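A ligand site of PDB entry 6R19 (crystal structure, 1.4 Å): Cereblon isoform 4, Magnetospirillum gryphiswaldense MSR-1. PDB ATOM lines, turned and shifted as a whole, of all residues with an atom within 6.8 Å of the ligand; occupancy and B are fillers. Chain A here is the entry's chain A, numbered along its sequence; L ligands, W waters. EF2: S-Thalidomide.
Pro 52 touches the ligand (CD to O01, 3.4 Å). O of Glu 77 touches O18 of the ligand (3.8 Å). Ser 79 touches the ligand. CZ2 of Trp 86 touches O18 of the ligand (3.4 Å). Trp 100 touches the ligand (NE1 to C07, 3.4 Å). Hydrophobic or aromatic side chains within 4 Å of the ligand: Pro 52, Phe 78, Trp 80, Trp 86, Trp 100 and Tyr 102. Within 4 Å of the ligand: Asn 51, Pro 52, Glu 77, Phe 78, Ser 79, Trp 80, Trp 86, Trp 100 and Tyr 102. The nearest printed residue that does not touch the ligand is Phe 57 (4.3 Å).
The side-chain amide oxygen of Asn 51 is in hydrogen-bond range of the backbone NH of Ala 53, at 3.0 Å. The side-chain amide oxygen (OD1) of Asn 51 sits at hydrogen-bond distance from the backbone NH (N) of Met 55, 2.9 Å away. The indole nitrogen (NE1) of Trp 80 sits at hydrogen-bond distance from the backbone carbonyl oxygen (O) of Phe 50 (2.9 Å). The indole nitrogen (NE1) of Trp 86 lies within hydrogen-bond range of the backbone carbonyl oxygen (O) of Glu 77, at 2.8 Å. The backbone NH (N) of Trp 86 is in hydrogen-bond range of the backbone carbonyl oxygen (O) of Ser 75, 2.8 Å away. The backbone carbonyl oxygen (O) of Phe 81 sits at hydrogen-bond distance from the side-chain hydroxyl (OG) of Ser 79, at 3.1 Å. OG of Ser 79 is in hydrogen-bond range of O of Tyr 84 (2.9 Å). The backbone NH (N) of Glu 77 sits at hydrogen-bond distance from the side-chain hydroxyl (OG) of Ser 75 (3.2 Å).
Water W2 bridges NE1 of Trp 100 (2.9 Å) and O16 of the ligand (3.4 Å).
An oxygen (O05) of the ligand is in hydrogen-bond range of the side-chain hydroxyl of Tyr 102, at 2.8 Å. The backbone carbonyl oxygen of Phe 78 lies within hydrogen-bond range of a nitrogen (N03) of the ligand. An oxygen (O16) of the ligand sits at hydrogen-bond distance from the side-chain amide nitrogen of Asn 51 (2.9 Å). The backbone NH of Trp 80 sits at hydrogen-bond distance from an oxygen (O05) of the ligand (3.1 Å).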
ATOM      1  N   VAL A  49      22.797   6.626  -0.993  1.00  0.00           N
ATOM      2  CA  VAL A  49      22.665   6.755   0.439  1.00  0.00           C
ATOM      3  C   VAL A  49      22.338   5.394   1.053  1.00  0.00           C
ATOM      4  O   VAL A  49      21.885   4.515   0.326  1.00  0.00           O
ATOM      5  CB  VAL A  49      21.560   7.761   0.803  1.00  0.00           C
ATOM      6  CG1 VAL A  49      21.984   9.148   0.257  1.00  0.00           C
ATOM      7  CG2 VAL A  49      20.201   7.336   0.246  1.00  0.00           C
ATOM      8  N   PHE A  50      22.584   5.231   2.371  1.00  0.00           N
ATOM      9  CA  PHE A  50      22.032   4.091   3.068  1.00  0.00           C
ATOM     10  C   PHE A  50      21.351   4.442   4.331  1.00  0.00           C
ATOM     11  O   PHE A  50      21.714   5.432   4.983  1.00  0.00           O
ATOM     12  CB  PHE A  50      23.074   2.959   3.311  1.00  0.00           C
ATOM     13  CG  PHE A  50      24.153   3.318   4.184  1.00  0.00           C
ATOM     14  CD1 PHE A  50      25.318   3.929   3.715  1.00  0.00           C
ATOM     15  CD2 PHE A  50      24.091   3.064   5.594  1.00  0.00           C
ATOM     16  CE1 PHE A  50      26.330   4.281   4.579  1.00  0.00           C
ATOM     17  CE2 PHE A  50      25.077   3.442   6.461  1.00  0.00           C
ATOM     18  CZ  PHE A  50      26.229   4.025   5.971  1.00  0.00           C
ATOM     19  N   ASN A  51      20.375   3.667   4.736  1.00  0.00           N
ATOM     20  CA  ASN A  51      19.632   3.894   5.976  1.00  0.00           C
ATOM     21  C   ASN A  51      20.225   3.058   7.148  1.00  0.00           C
ATOM     22  O   ASN A  51      21.163   2.275   6.965  1.00  0.00           O
ATOM     23  CB  ASN A  51      18.127   3.656   5.723  1.00  0.00           C
ATOM     24  CG  ASN A  51      17.785   2.194   5.501  1.00  0.00           C
ATOM     25  OD1 ASN A  51      18.582   1.278   5.714  1.00  0.00           O
ATOM     26  ND2 ASN A  51      16.518   1.985   5.205  1.00  0.00           N
ATOM     27  N   PRO A  52      19.677   3.212   8.353  1.00  0.00           N
ATOM     28  CA  PRO A  52      20.192   2.481   9.512  1.00  0.00           C
ATOM     29  C   PRO A  52      20.039   0.992   9.408  1.00  0.00           C
ATOM     30  O   PRO A  52      20.783   0.285  10.095  1.00  0.00           O
ATOM     31  CB  PRO A  52      19.378   3.034  10.690  1.00  0.00           C
ATOM     32  CG  PRO A  52      19.066   4.423  10.236  1.00  0.00           C
ATOM     33  CD  PRO A  52      18.717   4.276   8.784  1.00  0.00           C
ATOM     34  N   ALA A  53      19.163   0.497   8.547  1.00  0.00           N
ATOM     35  CA  ALA A  53      19.001  -0.936   8.301  1.00  0.00           C
ATOM     36  C   ALA A  53      19.964  -1.405   7.215  1.00  0.00           C
ATOM     37  O   ALA A  53      19.877  -2.531   6.767  1.00  0.00           O
ATOM     38  CB  ALA A  53      17.576  -1.271   7.927  1.00  0.00           C
ATOM     39  N   MET A  55      20.150  -0.526   4.048  1.00  0.00           N
ATOM     40  CA  MET A  55      19.609  -0.552   2.661  1.00  0.00           C
ATOM     41  C   MET A  55      20.211   0.612   1.908  1.00  0.00           C
ATOM     42  O   MET A  55      20.204   1.748   2.428  1.00  0.00           O
ATOM     43  CB  MET A  55      18.114  -0.480   2.670  1.00  0.00           C
ATOM     44  CG  MET A  55      17.487  -0.523   1.305  1.00  0.00           C
ATOM     45  SD  MET A  55      17.958  -1.895   0.237  1.00  0.00           S
ATOM     46  CE  MET A  55      17.524  -3.325   1.253  1.00  0.00           C
ATOM     47  N   PHE A  57      20.092   3.114  -1.352  1.00  0.00           N
ATOM     48  CA  PHE A  57      19.051   3.711  -2.248  1.00  0.00           C
ATOM     49  C   PHE A  57      19.765   4.644  -3.216  1.00  0.00           C
ATOM     50  O   PHE A  57      20.662   5.404  -2.833  1.00  0.00           O
ATOM     51  CB  PHE A  57      18.007   4.471  -1.525  1.00  0.00           C
ATOM     52  CG  PHE A  57      17.255   3.726  -0.453  1.00  0.00           C
ATOM     53  CD1 PHE A  57      16.187   2.955  -0.777  1.00  0.00           C
ATOM     54  CD2 PHE A  57      17.586   3.796   0.885  1.00  0.00           C
ATOM     55  CE1 PHE A  57      15.464   2.249   0.189  1.00  0.00           C
ATOM     56  CE2 PHE A  57      16.857   3.097   1.840  1.00  0.00           C
ATOM     57  CZ  PHE A  57      15.791   2.356   1.507  1.00  0.00           C
ATOM     58  N   SER A  75      10.752  14.277  10.508  1.00  0.00           N
ATOM     59  CA  SER A  75      11.818  13.957  11.399  1.00  0.00           C
ATOM     60  C   SER A  75      13.135  14.369  10.834  1.00  0.00           C
ATOM     61  O   SER A  75      13.367  14.158   9.629  1.00  0.00           O
ATOM     62  CB  SER A  75      11.833  12.424  11.631  1.00  0.00           C
ATOM     63  OG  SER A  75      12.927  12.076  12.499  1.00  0.00           O
ATOM     64  N   GLY A  76      14.041  14.901  11.621  1.00  0.00           N
ATOM     65  CA  GLY A  76      15.403  15.147  11.182  1.00  0.00           C
ATOM     66  C   GLY A  76      16.366  13.993  11.349  1.00  0.00           C
ATOM     67  O   GLY A  76      17.504  14.095  10.880  1.00  0.00           O
ATOM     68  N   GLU A  77      15.936  12.938  12.005  1.00  0.00           N
ATOM     69  CA  GLU A  77      16.830  11.831  12.356  1.00  0.00           C
ATOM     70  C   GLU A  77      17.387  11.181  11.114  1.00  0.00           C
ATOM     71  O   GLU A  77      16.673  10.844  10.212  1.00  0.00           O
ATOM     72  CB  GLU A  77      16.105  10.803  13.221  1.00  0.00           C
ATOM     73  CG  GLU A  77      15.629  11.381  14.531  1.00  0.00           C
ATOM     74  CD  GLU A  77      14.914  10.355  15.393  1.00  0.00           C
ATOM     75  OE1 GLU A  77      15.028   9.160  15.102  1.00  0.00           O
ATOM     76  OE2 GLU A  77      14.264  10.789  16.374  1.00  0.00           O
ATOM     77  N   PHE A  78      18.701  10.983  11.056  1.00  0.00           N
ATOM     78  CA  PHE A  78      19.385  10.273  10.005  1.00  0.00           C
ATOM     79  C   PHE A  78      19.203  10.968   8.647  1.00  0.00           C
ATOM     80  O   PHE A  78      19.459  10.375   7.610  1.00  0.00           O
ATOM     81  CB  PHE A  78      18.923   8.801   9.891  1.00  0.00           C
ATOM     82  CG  PHE A  78      18.962   8.038  11.184  1.00  0.00           C
ATOM     83  CD1 PHE A  78      20.113   7.792  11.789  1.00  0.00           C
ATOM     84  CD2 PHE A  78      17.785   7.595  11.732  1.00  0.00           C
ATOM     85  CE1 PHE A  78      20.179   7.046  12.960  1.00  0.00           C
ATOM     86  CE2 PHE A  78      17.785   6.899  12.923  1.00  0.00           C
ATOM     87  CZ  PHE A  78      18.982   6.622  13.521  1.00  0.00           C
ATOM     88  N   SER A  79      18.782  12.245   8.595  1.00  0.00           N
ATOM     89  CA  SER A  79      18.556  12.847   7.308  1.00  0.00           C
ATOM     90  C   SER A  79      19.798  12.885   6.453  1.00  0.00           C
ATOM     91  O   SER A  79      20.869  13.309   6.878  1.00  0.00           O
ATOM     92  CB  SER A  79      18.062  14.300   7.462  1.00  0.00           C
ATOM     93  OG  SER A  79      17.753  14.785   6.158  1.00  0.00           O
ATOM     94  N   TRP A  80      19.644  12.487   5.197  1.00  0.00           N
ATOM     95  CA  TRP A  80      20.705  12.455   4.203  1.00  0.00           C
ATOM     96  C   TRP A  80      20.993  13.854   3.678  1.00  0.00           C
ATOM     97  O   TRP A  80      21.996  14.056   2.957  1.00  0.00           O
ATOM     98  CB  TRP A  80      20.347  11.521   3.100  1.00  0.00           C
ATOM     99  CG  TRP A  80      20.258  10.111   3.519  1.00  0.00           C
ATOM    100  CD1 TRP A  80      21.168   9.347   4.187  1.00  0.00           C
ATOM    101  CD2 TRP A  80      19.194   9.218   3.149  1.00  0.00           C
ATOM    102  NE1 TRP A  80      20.716   8.048   4.328  1.00  0.00           N
ATOM    103  CE2 TRP A  80      19.510   7.946   3.669  1.00  0.00           C
ATOM    104  CE3 TRP A  80      18.000   9.366   2.410  1.00  0.00           C
ATOM    105  CZ2 TRP A  80      18.655   6.882   3.513  1.00  0.00           C
ATOM    106  CZ3 TRP A  80      17.184   8.304   2.273  1.00  0.00           C
ATOM    107  CH2 TRP A  80      17.529   7.062   2.797  1.00  0.00           C
ATOM    108  N   PHE A  81      20.154  14.837   3.960  1.00  0.00           N
ATOM    109  CA  PHE A  81      20.272  16.151   3.372  1.00  0.00           C
ATOM    110  C   PHE A  81      20.284  17.170   4.491  1.00  0.00           C
ATOM    111  O   PHE A  81      19.263  17.331   5.221  1.00  0.00           O
ATOM    112  CB  PHE A  81      19.118  16.408   2.363  1.00  0.00           C
ATOM    113  CG  PHE A  81      19.094  15.437   1.236  1.00  0.00           C
ATOM    114  CD1 PHE A  81      19.887  15.673   0.119  1.00  0.00           C
ATOM    115  CD2 PHE A  81      18.316  14.393   1.266  1.00  0.00           C
ATOM    116  CE1 PHE A  81      19.804  14.833  -1.013  1.00  0.00           C
ATOM    117  CE2 PHE A  81      18.282  13.471   0.194  1.00  0.00           C
ATOM    118  CZ  PHE A  81      19.038  13.695  -0.940  1.00  0.00           C
ATOM    119  N   TYR A  84      17.352  19.401   6.335  1.00  0.00           N
ATOM    120  CA  TYR A  84      16.007  18.965   5.983  1.00  0.00           C
ATOM    121  C   TYR A  84      15.513  17.864   6.878  1.00  0.00           C
ATOM    122  O   TYR A  84      16.263  17.019   7.317  1.00  0.00           O
ATOM    123  CB  TYR A  84      15.977  18.437   4.535  1.00  0.00           C
ATOM    124  CG  TYR A  84      16.269  19.463   3.498  1.00  0.00           C
ATOM    125  CD1 TYR A  84      15.278  20.247   2.938  1.00  0.00           C
ATOM    126  CD2 TYR A  84      17.559  19.629   3.060  1.00  0.00           C
ATOM    127  CE1 TYR A  84      15.579  21.200   1.950  1.00  0.00           C
ATOM    128  CE2 TYR A  84      17.863  20.578   2.104  1.00  0.00           C
ATOM    129  CZ  TYR A  84      16.891  21.350   1.563  1.00  0.00           C
ATOM    130  OH  TYR A  84      17.224  22.288   0.622  1.00  0.00           O
ATOM    131  N   TRP A  86      12.408  14.872   7.113  1.00  0.00           N
ATOM    132  CA  TRP A  86      11.761  13.977   6.096  1.00  0.00           C
ATOM    133  C   TRP A  86      10.465  13.404   6.609  1.00  0.00           C
ATOM    134  O   TRP A  86      10.285  13.188   7.810  1.00  0.00           O
ATOM    135  CB  TRP A  86      12.700  12.879   5.680  1.00  0.00           C
ATOM    136  CG  TRP A  86      13.285  12.095   6.743  1.00  0.00           C
ATOM    137  CD1 TRP A  86      14.488  12.309   7.331  1.00  0.00           C
ATOM    138  CD2 TRP A  86      12.708  10.980   7.442  1.00  0.00           C
ATOM    139  NE1 TRP A  86      14.683  11.420   8.345  1.00  0.00           N
ATOM    140  CE2 TRP A  86      13.588  10.620   8.481  1.00  0.00           C
ATOM    141  CE3 TRP A  86      11.508  10.264   7.310  1.00  0.00           C
ATOM    142  CZ2 TRP A  86      13.297   9.607   9.352  1.00  0.00           C
ATOM    143  CZ3 TRP A  86      11.254   9.229   8.185  1.00  0.00           C
ATOM    144  CH2 TRP A  86      12.148   8.897   9.190  1.00  0.00           C
ATOM    145  N   THR A  87       9.613  13.071   5.632  1.00  0.00           N
ATOM    146  CA  THR A  87       8.431  12.254   5.846  1.00  0.00           C
ATOM    147  C   THR A  87       8.462  11.184   4.791  1.00  0.00           C
ATOM    148  O   THR A  87       8.889  11.408   3.647  1.00  0.00           O
ATOM    149  CB  THR A  87       7.104  12.992   5.724  1.00  0.00           C
ATOM    150  OG1 THR A  87       7.001  13.675   4.484  1.00  0.00           O
ATOM    151  CG2 THR A  87       6.899  13.928   6.915  1.00  0.00           C
ATOM    152  N   ILE A  88       8.040  10.005   5.151  1.00  0.00           N
ATOM    153  CA  ILE A  88       7.946   8.898   4.179  1.00  0.00           C
ATOM    154  C   ILE A  88       6.921   9.251   3.125  1.00  0.00           C
ATOM    155  O   ILE A  88       5.800   9.735   3.456  1.00  0.00           O
ATOM    156  CB  ILE A  88       7.542   7.618   4.940  1.00  0.00           C
ATOM    157  CG1 ILE A  88       8.735   7.160   5.760  1.00  0.00           C
ATOM    158  CG2 ILE A  88       7.056   6.530   3.973  1.00  0.00           C
ATOM    159  CD1 ILE A  88       8.360   6.119   6.828  1.00  0.00           C
ATOM    160  N   HIS A  97       6.487   2.084  -1.158  1.00  0.00           N
ATOM    161  CA  HIS A  97       7.333   3.141  -0.628  1.00  0.00           C
ATOM    162  C   HIS A  97       8.221   3.709  -1.710  1.00  0.00           C
ATOM    163  O   HIS A  97       9.130   3.017  -2.157  1.00  0.00           O
ATOM    164  CB  HIS A  97       8.140   2.624   0.574  1.00  0.00           C
ATOM    165  CG  HIS A  97       9.082   3.626   1.075  1.00  0.00           C
ATOM    166  ND1 HIS A  97      10.288   3.258   1.683  1.00  0.00           N
ATOM    167  CD2 HIS A  97       9.012   4.971   1.095  1.00  0.00           C
ATOM    168  CE1 HIS A  97      10.888   4.387   2.026  1.00  0.00           C
ATOM    169  NE2 HIS A  97      10.137   5.431   1.710  1.00  0.00           N
ATOM    170  N   TRP A 100      10.868   9.887  -0.041  1.00  0.00           N
ATOM    171  CA  TRP A 100      10.657  10.773   1.111  1.00  0.00           C
ATOM    172  C   TRP A 100      10.392  12.159   0.577  1.00  0.00           C
ATOM    173  O   TRP A 100      10.908  12.558  -0.479  1.00  0.00           O
ATOM    174  CB  TRP A 100      11.915  10.795   2.012  1.00  0.00           C
ATOM    175  CG  TRP A 100      12.292   9.441   2.512  1.00  0.00           C
ATOM    176  CD1 TRP A 100      11.874   8.869   3.689  1.00  0.00           C
ATOM    177  CD2 TRP A 100      13.102   8.448   1.862  1.00  0.00           C
ATOM    178  NE1 TRP A 100      12.357   7.573   3.780  1.00  0.00           N
ATOM    179  CE2 TRP A 100      13.112   7.292   2.692  1.00  0.00           C
ATOM    180  CE3 TRP A 100      13.771   8.385   0.648  1.00  0.00           C
ATOM    181  CZ2 TRP A 100      13.835   6.142   2.340  1.00  0.00           C
ATOM    182  CZ3 TRP A 100      14.449   7.205   0.307  1.00  0.00           C
ATOM    183  CH2 TRP A 100      14.455   6.154   1.144  1.00  0.00           C
ATOM    184  N   TYR A 102      11.126  16.019   1.737  1.00  0.00           N
ATOM    185  CA  TYR A 102      12.020  16.786   2.630  1.00  0.00           C
ATOM    186  C   TYR A 102      11.485  18.212   2.750  1.00  0.00           C
ATOM    187  O   TYR A 102      10.993  18.784   1.776  1.00  0.00           O
ATOM    188  CB  TYR A 102      13.421  16.824   2.025  1.00  0.00           C
ATOM    189  CG  TYR A 102      14.095  15.451   2.127  1.00  0.00           C
ATOM    190  CD1 TYR A 102      14.730  15.079   3.317  1.00  0.00           C
ATOM    191  CD2 TYR A 102      14.012  14.524   1.095  1.00  0.00           C
ATOM    192  CE1 TYR A 102      15.327  13.810   3.406  1.00  0.00           C
ATOM    193  CE2 TYR A 102      14.589  13.286   1.204  1.00  0.00           C
ATOM    194  CZ  TYR A 102      15.205  12.938   2.383  1.00  0.00           C
ATOM    195  OH  TYR A 102      15.818  11.687   2.495  1.00  0.00           O
HETATM  196  O01 EF2 L   1      17.982   7.020   6.847  1.00  0.00           O
HETATM  197  C02 EF2 L   1      17.127   7.776   6.347  1.00  0.00           C
HETATM  198  N03 EF2 L   1      17.422   9.075   6.019  1.00  0.00           N
HETATM  199  C04 EF2 L   1      16.558   9.945   5.351  1.00  0.00           C
HETATM  200  O05 EF2 L   1      16.958  11.004   4.932  1.00  0.00           O
HETATM  201  C06 EF2 L   1      15.185   9.377   5.119  1.00  0.00           C
HETATM  202  C07 EF2 L   1      14.734   8.361   6.141  1.00  0.00           C
HETATM  203  C08 EF2 L   1      15.728   7.250   6.036  1.00  0.00           C
HETATM  204  N09 EF2 L   1      15.449   6.166   6.965  1.00  0.00           N
HETATM  205  C11 EF2 L   1      14.705   2.270   9.235  1.00  0.00           C
HETATM  206  C12 EF2 L   1      14.768   2.742   7.931  1.00  0.00           C
HETATM  207  C13 EF2 L   1      15.032   4.086   7.775  1.00  0.00           C
HETATM  208  C14 EF2 L   1      15.217   4.916   8.887  1.00  0.00           C
HETATM  209  O16 EF2 L   1      15.109   4.556   5.446  1.00  0.00           O
HETATM  210  O18 EF2 L   1      15.761   7.300   9.018  1.00  0.00           O
HETATM  211  C19 EF2 L   1      15.138   4.459  10.182  1.00  0.00           C
HETATM  212  C20 EF2 L   1      14.872   3.097  10.354  1.00  0.00           C
HETATM  213  C3  EF2 L   1      15.458   6.134   8.294  1.00  0.00           C
HETATM  214  C4  EF2 L   1      15.135   4.893   6.651  1.00  0.00           C
HETATM  215  O   HOH W   1      14.223   7.380  11.698  1.00  0.00           O
HETATM  216  O   HOH W   2      11.958   5.782   6.007  1.00  0.00           O
HETATM  217  O   HOH W   3      13.038   3.223   4.298  1.00  0.00           O
